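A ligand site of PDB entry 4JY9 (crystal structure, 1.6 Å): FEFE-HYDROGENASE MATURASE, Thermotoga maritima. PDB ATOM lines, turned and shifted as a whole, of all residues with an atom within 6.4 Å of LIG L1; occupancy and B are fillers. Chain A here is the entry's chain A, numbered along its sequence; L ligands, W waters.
The side-chain sulfur (SG) of Cys 70 sits close to the backbone NH (N) of Leu 72 (3.4 Å).
N of Lys 65 lies close to SG of Cys 63 (3.4 Å).
The backbone NH (N) of Glu 110 lies close to the side-chain sulfur (SG) of Cys 63.
NE of Arg 73 is in hydrogen-bond range of O of Cys 67, 3.0 Å away.
The backbone carbonyl oxygen (O) of Asn 66 is in hydrogen-bond range of the guanidinium group (NH2) of Arg 73 (2.9 Å).
The side-chain hydroxyl (OH) of Tyr 69 is in hydrogen-bond range of the guanidinium group (NE) of Arg 172 (3.0 Å).
The side-chain amino group of Lys 65 lies within salt-bridge range of the side-chain carboxylate of Glu 110, 2.7 Å away.
The guanidinium group (NE) of Arg 64 is in salt-bridge range of the side-chain carboxylate (OE1) of Glu 110 (2.8 Å).
An iron atom (FE4) of LIG L1 is bound by the side-chain sulfur of Cys 70, at 2.3 Å.
The side-chain sulfur of Cys 63 is bound to an iron atom (FE3) of LIG L1.
A sulfur (S2) of LIG L1 lies close to the backbone NH (N) of Cys 67 (3.8 Å).
FE1 of LIG L1 is bound by SG of Cys 67 (2.4 Å).
O of Tyr 69 is in hydrogen-bond range of N4 of LG2 L2 (2.9 Å).
The backbone carbonyl oxygen (O) of Ser 108 sits close to a nitrogen (N1) of LG2 L2, at 3.1 Å.
OE2 of Glu 161 sits at hydrogen-bond distance from O4 of LG2 L2.
The guanidinium group (NH2) of Arg 180 is in salt-bridge range of an oxygen (O2) of LG2 L2 (3.0 Å).
Water W2 lies within hydrogen-bond range of OH of Tyr 69 (2.7 Å), OE2 of Glu 161 (2.8 Å), NE of Arg 172 (3.1 Å) and S3 of LIG L1 (3.2 Å).
Water W1 lies within hydrogen-bond range of OE2 of Glu 110 (2.7 Å), NH1 of Arg 180 (2.7 Å), NH2 of Arg 172 (3.3 Å) and S4 of LIG L1 (3.3 Å).
CB of Lys 65 touches S4 of LIG L1 (3.9 Å).
Tyr 69 touches LIG L1 (CE1 to S3, 3.8 Å).
Arg 73 touches LIG L1 (CA to S2, 3.7 Å).
Gly 109 touches LIG L1.
CG of Glu 110 touches S4 of LIG L1, 3.9 Å away.
Hydrophobic or aromatic side chains that line LIG L1: Tyr 69.
Of the 22 residues printed, 8 come within 4 Å of LIG L1.
FE2 of LIG L1 is bound by O1 of LG2 L2, 2.2 Å away.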
ATOM      1  N   VAL A  62      12.200   4.294 -11.278  1.00  0.00           N
ATOM      2  CA  VAL A  62      11.388   3.226 -11.854  1.00  0.00           C
ATOM      3  C   VAL A  62      11.565   3.282 -13.384  1.00  0.00           C
ATOM      4  O   VAL A  62      11.464   4.356 -13.986  1.00  0.00           O
ATOM      5  CB  VAL A  62       9.911   3.366 -11.467  1.00  0.00           C
ATOM      6  CG1 VAL A  62       8.988   2.358 -12.255  1.00  0.00           C
ATOM      7  CG2 VAL A  62       9.731   3.252  -9.984  1.00  0.00           C
ATOM      8  N   CYS A  63      11.860   2.138 -14.023  1.00  0.00           N
ATOM      9  CA  CYS A  63      11.896   2.088 -15.455  1.00  0.00           C
ATOM     10  C   CYS A  63      11.266   0.853 -16.030  1.00  0.00           C
ATOM     11  O   CYS A  63      11.407  -0.247 -15.484  1.00  0.00           O
ATOM     12  CB  CYS A  63      13.341   2.172 -15.971  1.00  0.00           C
ATOM     13  SG  CYS A  63      13.405   2.606 -17.731  1.00  0.00           S
ATOM     14  N   ARG A  64      10.536   1.046 -17.121  1.00  0.00           N
ATOM     15  CA  ARG A  64       9.886  -0.025 -17.892  1.00  0.00           C
ATOM     16  C   ARG A  64      10.820  -0.668 -18.957  1.00  0.00           C
ATOM     17  O   ARG A  64      10.477  -1.728 -19.484  1.00  0.00           O
ATOM     18  CB  ARG A  64       8.655   0.524 -18.609  1.00  0.00           C
ATOM     19  CG  ARG A  64       9.008   1.487 -19.760  1.00  0.00           C
ATOM     20  CD  ARG A  64       7.777   2.158 -20.322  1.00  0.00           C
ATOM     21  NE  ARG A  64       8.105   3.114 -21.326  1.00  0.00           N
ATOM     22  CZ  ARG A  64       7.282   3.523 -22.296  1.00  0.00           C
ATOM     23  NH1 ARG A  64       6.018   3.083 -22.433  1.00  0.00           N
ATOM     24  NH2 ARG A  64       7.731   4.357 -23.167  1.00  0.00           N
ATOM     25  N   LYS A  65      11.928  -0.007 -19.299  1.00  0.00           N
ATOM     26  CA  LYS A  65      12.849  -0.530 -20.291  1.00  0.00           C
ATOM     27  C   LYS A  65      13.978  -1.324 -19.656  1.00  0.00           C
ATOM     28  O   LYS A  65      14.124  -1.376 -18.437  1.00  0.00           O
ATOM     29  CB  LYS A  65      13.401   0.609 -21.176  1.00  0.00           C
ATOM     30  CG  LYS A  65      12.408   1.079 -22.255  1.00  0.00           C
ATOM     31  CD  LYS A  65      13.071   2.124 -23.158  1.00  0.00           C
ATOM     32  CE  LYS A  65      12.305   2.346 -24.452  1.00  0.00           C
ATOM     33  NZ  LYS A  65      10.874   2.689 -24.240  1.00  0.00           N
ATOM     34  N   ASN A  66      14.736  -2.024 -20.511  1.00  0.00           N
ATOM     35  CA  ASN A  66      15.701  -2.991 -20.050  1.00  0.00           C
ATOM     36  C   ASN A  66      17.066  -2.778 -20.712  1.00  0.00           C
ATOM     37  O   ASN A  66      17.798  -3.764 -20.968  1.00  0.00           O
ATOM     38  CB  ASN A  66      15.141  -4.419 -20.329  1.00  0.00           C
ATOM     39  CG  ASN A  66      15.610  -5.454 -19.324  1.00  0.00           C
ATOM     40  OD1 ASN A  66      15.975  -5.134 -18.188  1.00  0.00           O
ATOM     41  ND2 ASN A  66      15.567  -6.733 -19.734  1.00  0.00           N
ATOM     42  N   CYS A  67      17.466  -1.536 -20.932  1.00  0.00           N
ATOM     43  CA  CYS A  67      18.756  -1.221 -21.558  1.00  0.00           C
ATOM     44  C   CYS A  67      19.886  -1.991 -20.920  1.00  0.00           C
ATOM     45  O   CYS A  67      19.982  -2.049 -19.698  1.00  0.00           O
ATOM     46  CB  CYS A  67      19.014   0.280 -21.555  1.00  0.00           C
ATOM     47  SG  CYS A  67      17.645   1.240 -22.283  1.00  0.00           S
ATOM     48  N   LEU A  68      20.726  -2.638 -21.746  1.00  0.00           N
ATOM     49  CA  LEU A  68      21.705  -3.569 -21.160  1.00  0.00           C
ATOM     50  C   LEU A  68      22.777  -2.920 -20.313  1.00  0.00           C
ATOM     51  O   LEU A  68      23.374  -3.561 -19.470  1.00  0.00           O
ATOM     52  CB  LEU A  68      22.381  -4.413 -22.256  1.00  0.00           C
ATOM     53  CG  LEU A  68      21.643  -5.704 -22.694  1.00  0.00           C
ATOM     54  CD1 LEU A  68      20.241  -5.509 -23.187  1.00  0.00           C
ATOM     55  CD2 LEU A  68      22.532  -6.423 -23.739  1.00  0.00           C
ATOM     56  N   TYR A  69      23.032  -1.639 -20.574  1.00  0.00           N
ATOM     57  CA  TYR A  69      24.077  -0.867 -19.871  1.00  0.00           C
ATOM     58  C   TYR A  69      23.667  -0.255 -18.551  1.00  0.00           C
ATOM     59  O   TYR A  69      24.526   0.112 -17.716  1.00  0.00           O
ATOM     60  CB  TYR A  69      24.667   0.231 -20.778  1.00  0.00           C
ATOM     61  CG  TYR A  69      23.630   1.054 -21.461  1.00  0.00           C
ATOM     62  CD1 TYR A  69      22.952   2.075 -20.801  1.00  0.00           C
ATOM     63  CD2 TYR A  69      23.295   0.796 -22.798  1.00  0.00           C
ATOM     64  CE1 TYR A  69      21.994   2.795 -21.468  1.00  0.00           C
ATOM     65  CE2 TYR A  69      22.286   1.489 -23.458  1.00  0.00           C
ATOM     66  CZ  TYR A  69      21.675   2.508 -22.788  1.00  0.00           C
ATOM     67  OH  TYR A  69      20.707   3.204 -23.480  1.00  0.00           O
ATOM     68  N   CYS A  70      22.352  -0.158 -18.329  1.00  0.00           N
ATOM     69  CA  CYS A  70      21.823   0.753 -17.280  1.00  0.00           C
ATOM     70  C   CYS A  70      21.412   0.050 -15.989  1.00  0.00           C
ATOM     71  O   CYS A  70      20.655  -0.900 -16.017  1.00  0.00           O
ATOM     72  CB  CYS A  70      20.604   1.465 -17.842  1.00  0.00           C
ATOM     73  SG  CYS A  70      19.970   2.761 -16.736  1.00  0.00           S
ATOM     74  N   GLY A  71      21.884   0.547 -14.845  1.00  0.00           N
ATOM     75  CA  GLY A  71      21.528   0.044 -13.574  1.00  0.00           C
ATOM     76  C   GLY A  71      20.056   0.163 -13.212  1.00  0.00           C
ATOM     77  O   GLY A  71      19.571  -0.601 -12.380  1.00  0.00           O
ATOM     78  N   LEU A  72      19.308   1.033 -13.876  1.00  0.00           N
ATOM     79  CA  LEU A  72      17.847   1.161 -13.641  1.00  0.00           C
ATOM     80  C   LEU A  72      17.022   0.207 -14.503  1.00  0.00           C
ATOM     81  O   LEU A  72      15.804   0.168 -14.360  1.00  0.00           O
ATOM     82  CB  LEU A  72      17.371   2.607 -13.882  1.00  0.00           C
ATOM     83  CG  LEU A  72      18.032   3.724 -13.091  1.00  0.00           C
ATOM     84  CD1 LEU A  72      17.176   4.986 -13.163  1.00  0.00           C
ATOM     85  CD2 LEU A  72      18.532   3.410 -11.743  1.00  0.00           C
ATOM     86  N   ARG A  73      17.674  -0.613 -15.328  1.00  0.00           N
ATOM     87  CA  ARG A  73      16.910  -1.528 -16.221  1.00  0.00           C
ATOM     88  C   ARG A  73      15.932  -2.371 -15.400  1.00  0.00           C
ATOM     89  O   ARG A  73      16.195  -2.748 -14.252  1.00  0.00           O
ATOM     90  CB  ARG A  73      17.853  -2.472 -16.993  1.00  0.00           C
ATOM     91  CG  ARG A  73      18.719  -3.433 -16.131  1.00  0.00           C
ATOM     92  CD  ARG A  73      19.904  -3.977 -16.870  1.00  0.00           C
ATOM     93  NE  ARG A  73      19.506  -4.533 -18.122  1.00  0.00           N
ATOM     94  CZ  ARG A  73      19.189  -5.795 -18.402  1.00  0.00           C
ATOM     95  NH1 ARG A  73      19.168  -6.711 -17.459  1.00  0.00           N
ATOM     96  NH2 ARG A  73      18.827  -6.097 -19.646  1.00  0.00           N
ATOM     97  N   ARG A  74      14.795  -2.684 -16.012  1.00  0.00           N
ATOM     98  CA  ARG A  74      13.717  -3.331 -15.261  1.00  0.00           C
ATOM     99  C   ARG A  74      14.082  -4.641 -14.600  1.00  0.00           C
ATOM    100  O   ARG A  74      13.583  -4.946 -13.492  1.00  0.00           O
ATOM    101  CB  ARG A  74      12.444  -3.477 -16.050  1.00  0.00           C
ATOM    102  CG  ARG A  74      12.550  -4.294 -17.246  1.00  0.00           C
ATOM    103  CD  ARG A  74      11.139  -4.679 -17.841  1.00  0.00           C
ATOM    104  NE  ARG A  74      11.417  -5.663 -18.871  1.00  0.00           N
ATOM    105  CZ  ARG A  74      11.650  -5.363 -20.153  1.00  0.00           C
ATOM    106  NH1 ARG A  74      11.525  -4.119 -20.653  1.00  0.00           N
ATOM    107  NH2 ARG A  74      12.012  -6.316 -21.006  1.00  0.00           N
ATOM    108  N   SER A 108      14.310  10.982 -15.122  1.00  0.00           N
ATOM    109  CA  SER A 108      13.830   9.758 -14.504  1.00  0.00           C
ATOM    110  C   SER A 108      14.063   8.557 -15.417  1.00  0.00           C
ATOM    111  O   SER A 108      14.355   8.669 -16.642  1.00  0.00           O
ATOM    112  CB  SER A 108      12.352   9.859 -14.179  1.00  0.00           C
ATOM    113  OG  SER A 108      11.560  10.042 -15.360  1.00  0.00           O
ATOM    114  N   GLY A 109      13.912   7.386 -14.802  1.00  0.00           N
ATOM    115  CA  GLY A 109      13.624   6.191 -15.593  1.00  0.00           C
ATOM    116  C   GLY A 109      12.326   6.421 -16.364  1.00  0.00           C
ATOM    117  O   GLY A 109      11.545   7.350 -16.072  1.00  0.00           O
ATOM    118  N   GLU A 110      12.041   5.563 -17.323  1.00  0.00           N
ATOM    119  CA  GLU A 110      10.746   5.603 -18.035  1.00  0.00           C
ATOM    120  C   GLU A 110       9.692   5.013 -17.143  1.00  0.00           C
ATOM    121  O   GLU A 110       9.327   3.835 -17.248  1.00  0.00           O
ATOM    122  CB  GLU A 110      10.828   4.893 -19.382  1.00  0.00           C
ATOM    123  CG  GLU A 110      11.759   5.559 -20.406  1.00  0.00           C
ATOM    124  CD  GLU A 110      11.497   5.080 -21.832  1.00  0.00           C
ATOM    125  OE1 GLU A 110      10.575   4.238 -22.053  1.00  0.00           O
ATOM    126  OE2 GLU A 110      12.253   5.551 -22.714  1.00  0.00           O
ATOM    127  N   GLY A 138      12.968  10.034 -21.371  1.00  0.00           N
ATOM    128  CA  GLY A 138      13.004   8.909 -22.304  1.00  0.00           C
ATOM    129  C   GLY A 138      12.020   9.045 -23.462  1.00  0.00           C
ATOM    130  O   GLY A 138      11.619  10.167 -23.870  1.00  0.00           O
ATOM    131  N   GLU A 161      22.607   7.767 -27.849  1.00  0.00           N
ATOM    132  CA  GLU A 161      23.344   6.621 -27.219  1.00  0.00           C
ATOM    133  C   GLU A 161      24.423   6.043 -28.156  1.00  0.00           C
ATOM    134  O   GLU A 161      25.592   5.973 -27.808  1.00  0.00           O
ATOM    135  CB  GLU A 161      22.415   5.515 -26.713  1.00  0.00           C
ATOM    136  CG  GLU A 161      21.217   6.009 -25.921  1.00  0.00           C
ATOM    137  CD  GLU A 161      21.544   6.738 -24.619  1.00  0.00           C
ATOM    138  OE1 GLU A 161      22.706   6.947 -24.270  1.00  0.00           O
ATOM    139  OE2 GLU A 161      20.602   7.073 -23.900  1.00  0.00           O
ATOM    140  N   ARG A 172      19.515  -1.903 -26.532  1.00  0.00           N
ATOM    141  CA  ARG A 172      18.250  -1.279 -26.133  1.00  0.00           C
ATOM    142  C   ARG A 172      17.103  -2.088 -26.754  1.00  0.00           C
ATOM    143  O   ARG A 172      16.410  -1.656 -27.658  1.00  0.00           O
ATOM    144  CB  ARG A 172      18.233   0.178 -26.481  1.00  0.00           C
ATOM    145  CG  ARG A 172      19.455   0.912 -26.026  1.00  0.00           C
ATOM    146  CD  ARG A 172      19.373   2.426 -26.254  1.00  0.00           C
ATOM    147  NE  ARG A 172      18.368   2.967 -25.339  1.00  0.00           N
ATOM    148  CZ  ARG A 172      17.198   3.489 -25.688  1.00  0.00           C
ATOM    149  NH1 ARG A 172      16.903   3.736 -26.957  1.00  0.00           N
ATOM    150  NH2 ARG A 172      16.304   3.784 -24.731  1.00  0.00           N
ATOM    151  N   ARG A 180      14.358   6.199 -31.654  1.00  0.00           N
ATOM    152  CA  ARG A 180      15.092   7.249 -30.908  1.00  0.00           C
ATOM    153  C   ARG A 180      15.219   8.504 -31.762  1.00  0.00           C
ATOM    154  O   ARG A 180      14.971   9.629 -31.283  1.00  0.00           O
ATOM    155  CB  ARG A 180      16.472   6.720 -30.516  1.00  0.00           C
ATOM    156  CG  ARG A 180      17.182   7.520 -29.450  1.00  0.00           C
ATOM    157  CD  ARG A 180      16.585   7.201 -28.111  1.00  0.00           C
ATOM    158  NE  ARG A 180      17.375   7.691 -26.955  1.00  0.00           N
ATOM    159  CZ  ARG A 180      16.992   7.574 -25.678  1.00  0.00           C
ATOM    160  NH1 ARG A 180      15.894   6.920 -25.379  1.00  0.00           N
ATOM    161  NH2 ARG A 180      17.697   8.097 -24.686  1.00  0.00           N
ATOM    162  N   TYR A 303      19.729   6.297  -7.439  1.00  0.00           N
ATOM    163  CA  TYR A 303      19.659   6.595  -8.876  1.00  0.00           C
ATOM    164  C   TYR A 303      20.970   6.154  -9.527  1.00  0.00           C
ATOM    165  O   TYR A 303      21.831   6.916  -9.761  1.00  0.00           O
ATOM    166  CB  TYR A 303      19.296   8.061  -9.102  1.00  0.00           C
ATOM    167  CG  TYR A 303      18.889   8.339 -10.513  1.00  0.00           C
ATOM    168  CD1 TYR A 303      17.548   8.123 -10.933  1.00  0.00           C
ATOM    169  CD2 TYR A 303      19.806   8.793 -11.463  1.00  0.00           C
ATOM    170  CE1 TYR A 303      17.134   8.403 -12.211  1.00  0.00           C
ATOM    171  CE2 TYR A 303      19.360   9.057 -12.736  1.00  0.00           C
ATOM    172  CZ  TYR A 303      18.036   8.844 -13.106  1.00  0.00           C
ATOM    173  OH  TYR A 303      17.614   9.126 -14.394  1.00  0.00           O
ATOM    174  N   LEU A 305      22.539   4.672 -12.277  1.00  0.00           N
ATOM    175  CA  LEU A 305      22.676   4.338 -13.750  1.00  0.00           C
ATOM    176  C   LEU A 305      23.967   3.514 -13.892  1.00  0.00           C
ATOM    177  O   LEU A 305      24.023   2.560 -14.621  1.00  0.00           O
ATOM    178  CB  LEU A 305      22.759   5.589 -14.633  1.00  0.00           C
ATOM    179  CG  LEU A 305      21.572   6.568 -14.531  1.00  0.00           C
ATOM    180  CD1 LEU A 305      21.992   7.902 -15.187  1.00  0.00           C
ATOM    181  CD2 LEU A 305      20.305   6.022 -15.146  1.00  0.00           C
HETATM  182 FE1  LIG L   1      17.208   2.694 -20.474  1.00  0.00          FE
HETATM  183 FE2  LIG L   1      16.868   5.359 -19.477  1.00  0.00          FE
HETATM  184 FE3  LIG L   1      15.532   3.074 -18.374  1.00  0.00          FE
HETATM  185 FE4  LIG L   1      18.174   3.316 -18.001  1.00  0.00          FE
HETATM  186  S1  LIG L   1      16.625   4.735 -17.194  1.00  0.00           S
HETATM  187  S2  LIG L   1      17.008   1.390 -18.567  1.00  0.00           S
HETATM  188  S3  LIG L   1      18.853   4.280 -19.987  1.00  0.00           S
HETATM  189  S4  LIG L   1      15.319   3.910 -20.514  1.00  0.00           S
HETATM  190  N1  LG2 L   2      15.469   7.142 -19.041  1.00  0.00           N
HETATM  191  C1  LG2 L   2      15.920   8.377 -19.734  1.00  0.00           C
HETATM  192  C2  LG2 L   2      16.710   9.282 -18.817  1.00  0.00           C
HETATM  193  C3  LG2 L   2      17.591   8.549 -17.817  1.00  0.00           C
HETATM  194  S1  LG2 L   2      18.969   7.627 -18.471  1.00  0.00           S
HETATM  195  C4  LG2 L   2      16.678   7.987 -21.007  1.00  0.00           C
HETATM  196  O1  LG2 L   2      17.088   6.772 -21.185  1.00  0.00           O
HETATM  197  O2  LG2 L   2      16.908   8.821 -21.878  1.00  0.00           O
HETATM  198  C5  LG2 L   2      20.165   9.012 -18.707  1.00  0.00           C
HETATM  199  C6  LG2 L   2      21.455   8.715 -19.539  1.00  0.00           C
HETATM  200  O3  LG2 L   2      22.322   7.937 -18.703  1.00  0.00           O
HETATM  201  C7  LG2 L   2      21.329   7.823 -20.778  1.00  0.00           C
HETATM  202  O4  LG2 L   2      20.912   8.482 -21.925  1.00  0.00           O
HETATM  203  C8  LG2 L   2      22.698   7.124 -20.900  1.00  0.00           C
HETATM  204  O5  LG2 L   2      23.520   7.699 -21.922  1.00  0.00           O
HETATM  205  C9  LG2 L   2      23.362   7.345 -19.502  1.00  0.00           C
HETATM  206  N2  LG2 L   2      23.742   6.048 -18.895  1.00  0.00           N
HETATM  207  C10 LG2 L   2      22.900   5.003 -18.601  1.00  0.00           C
HETATM  208  N3  LG2 L   2      23.615   3.961 -18.131  1.00  0.00           N
HETATM  209  C11 LG2 L   2      24.948   4.299 -18.237  1.00  0.00           C
HETATM  210  C12 LG2 L   2      26.211   3.668 -17.912  1.00  0.00           C
HETATM  211  N4  LG2 L   2      26.219   2.402 -17.489  1.00  0.00           N
HETATM  212  N5  LG2 L   2      27.377   4.352 -18.167  1.00  0.00           N
HETATM  213  C13 LG2 L   2      27.367   5.652 -18.598  1.00  0.00           C
HETATM  214  N6  LG2 L   2      26.225   6.314 -18.848  1.00  0.00           N
HETATM  215  C14 LG2 L   2      25.031   5.674 -18.718  1.00  0.00           C
HETATM  216  O   HOH W   1      14.837   6.105 -22.987  1.00  0.00           O
HETATM  217  O   HOH W   2      18.793   5.122 -23.109  1.00  0.00           O
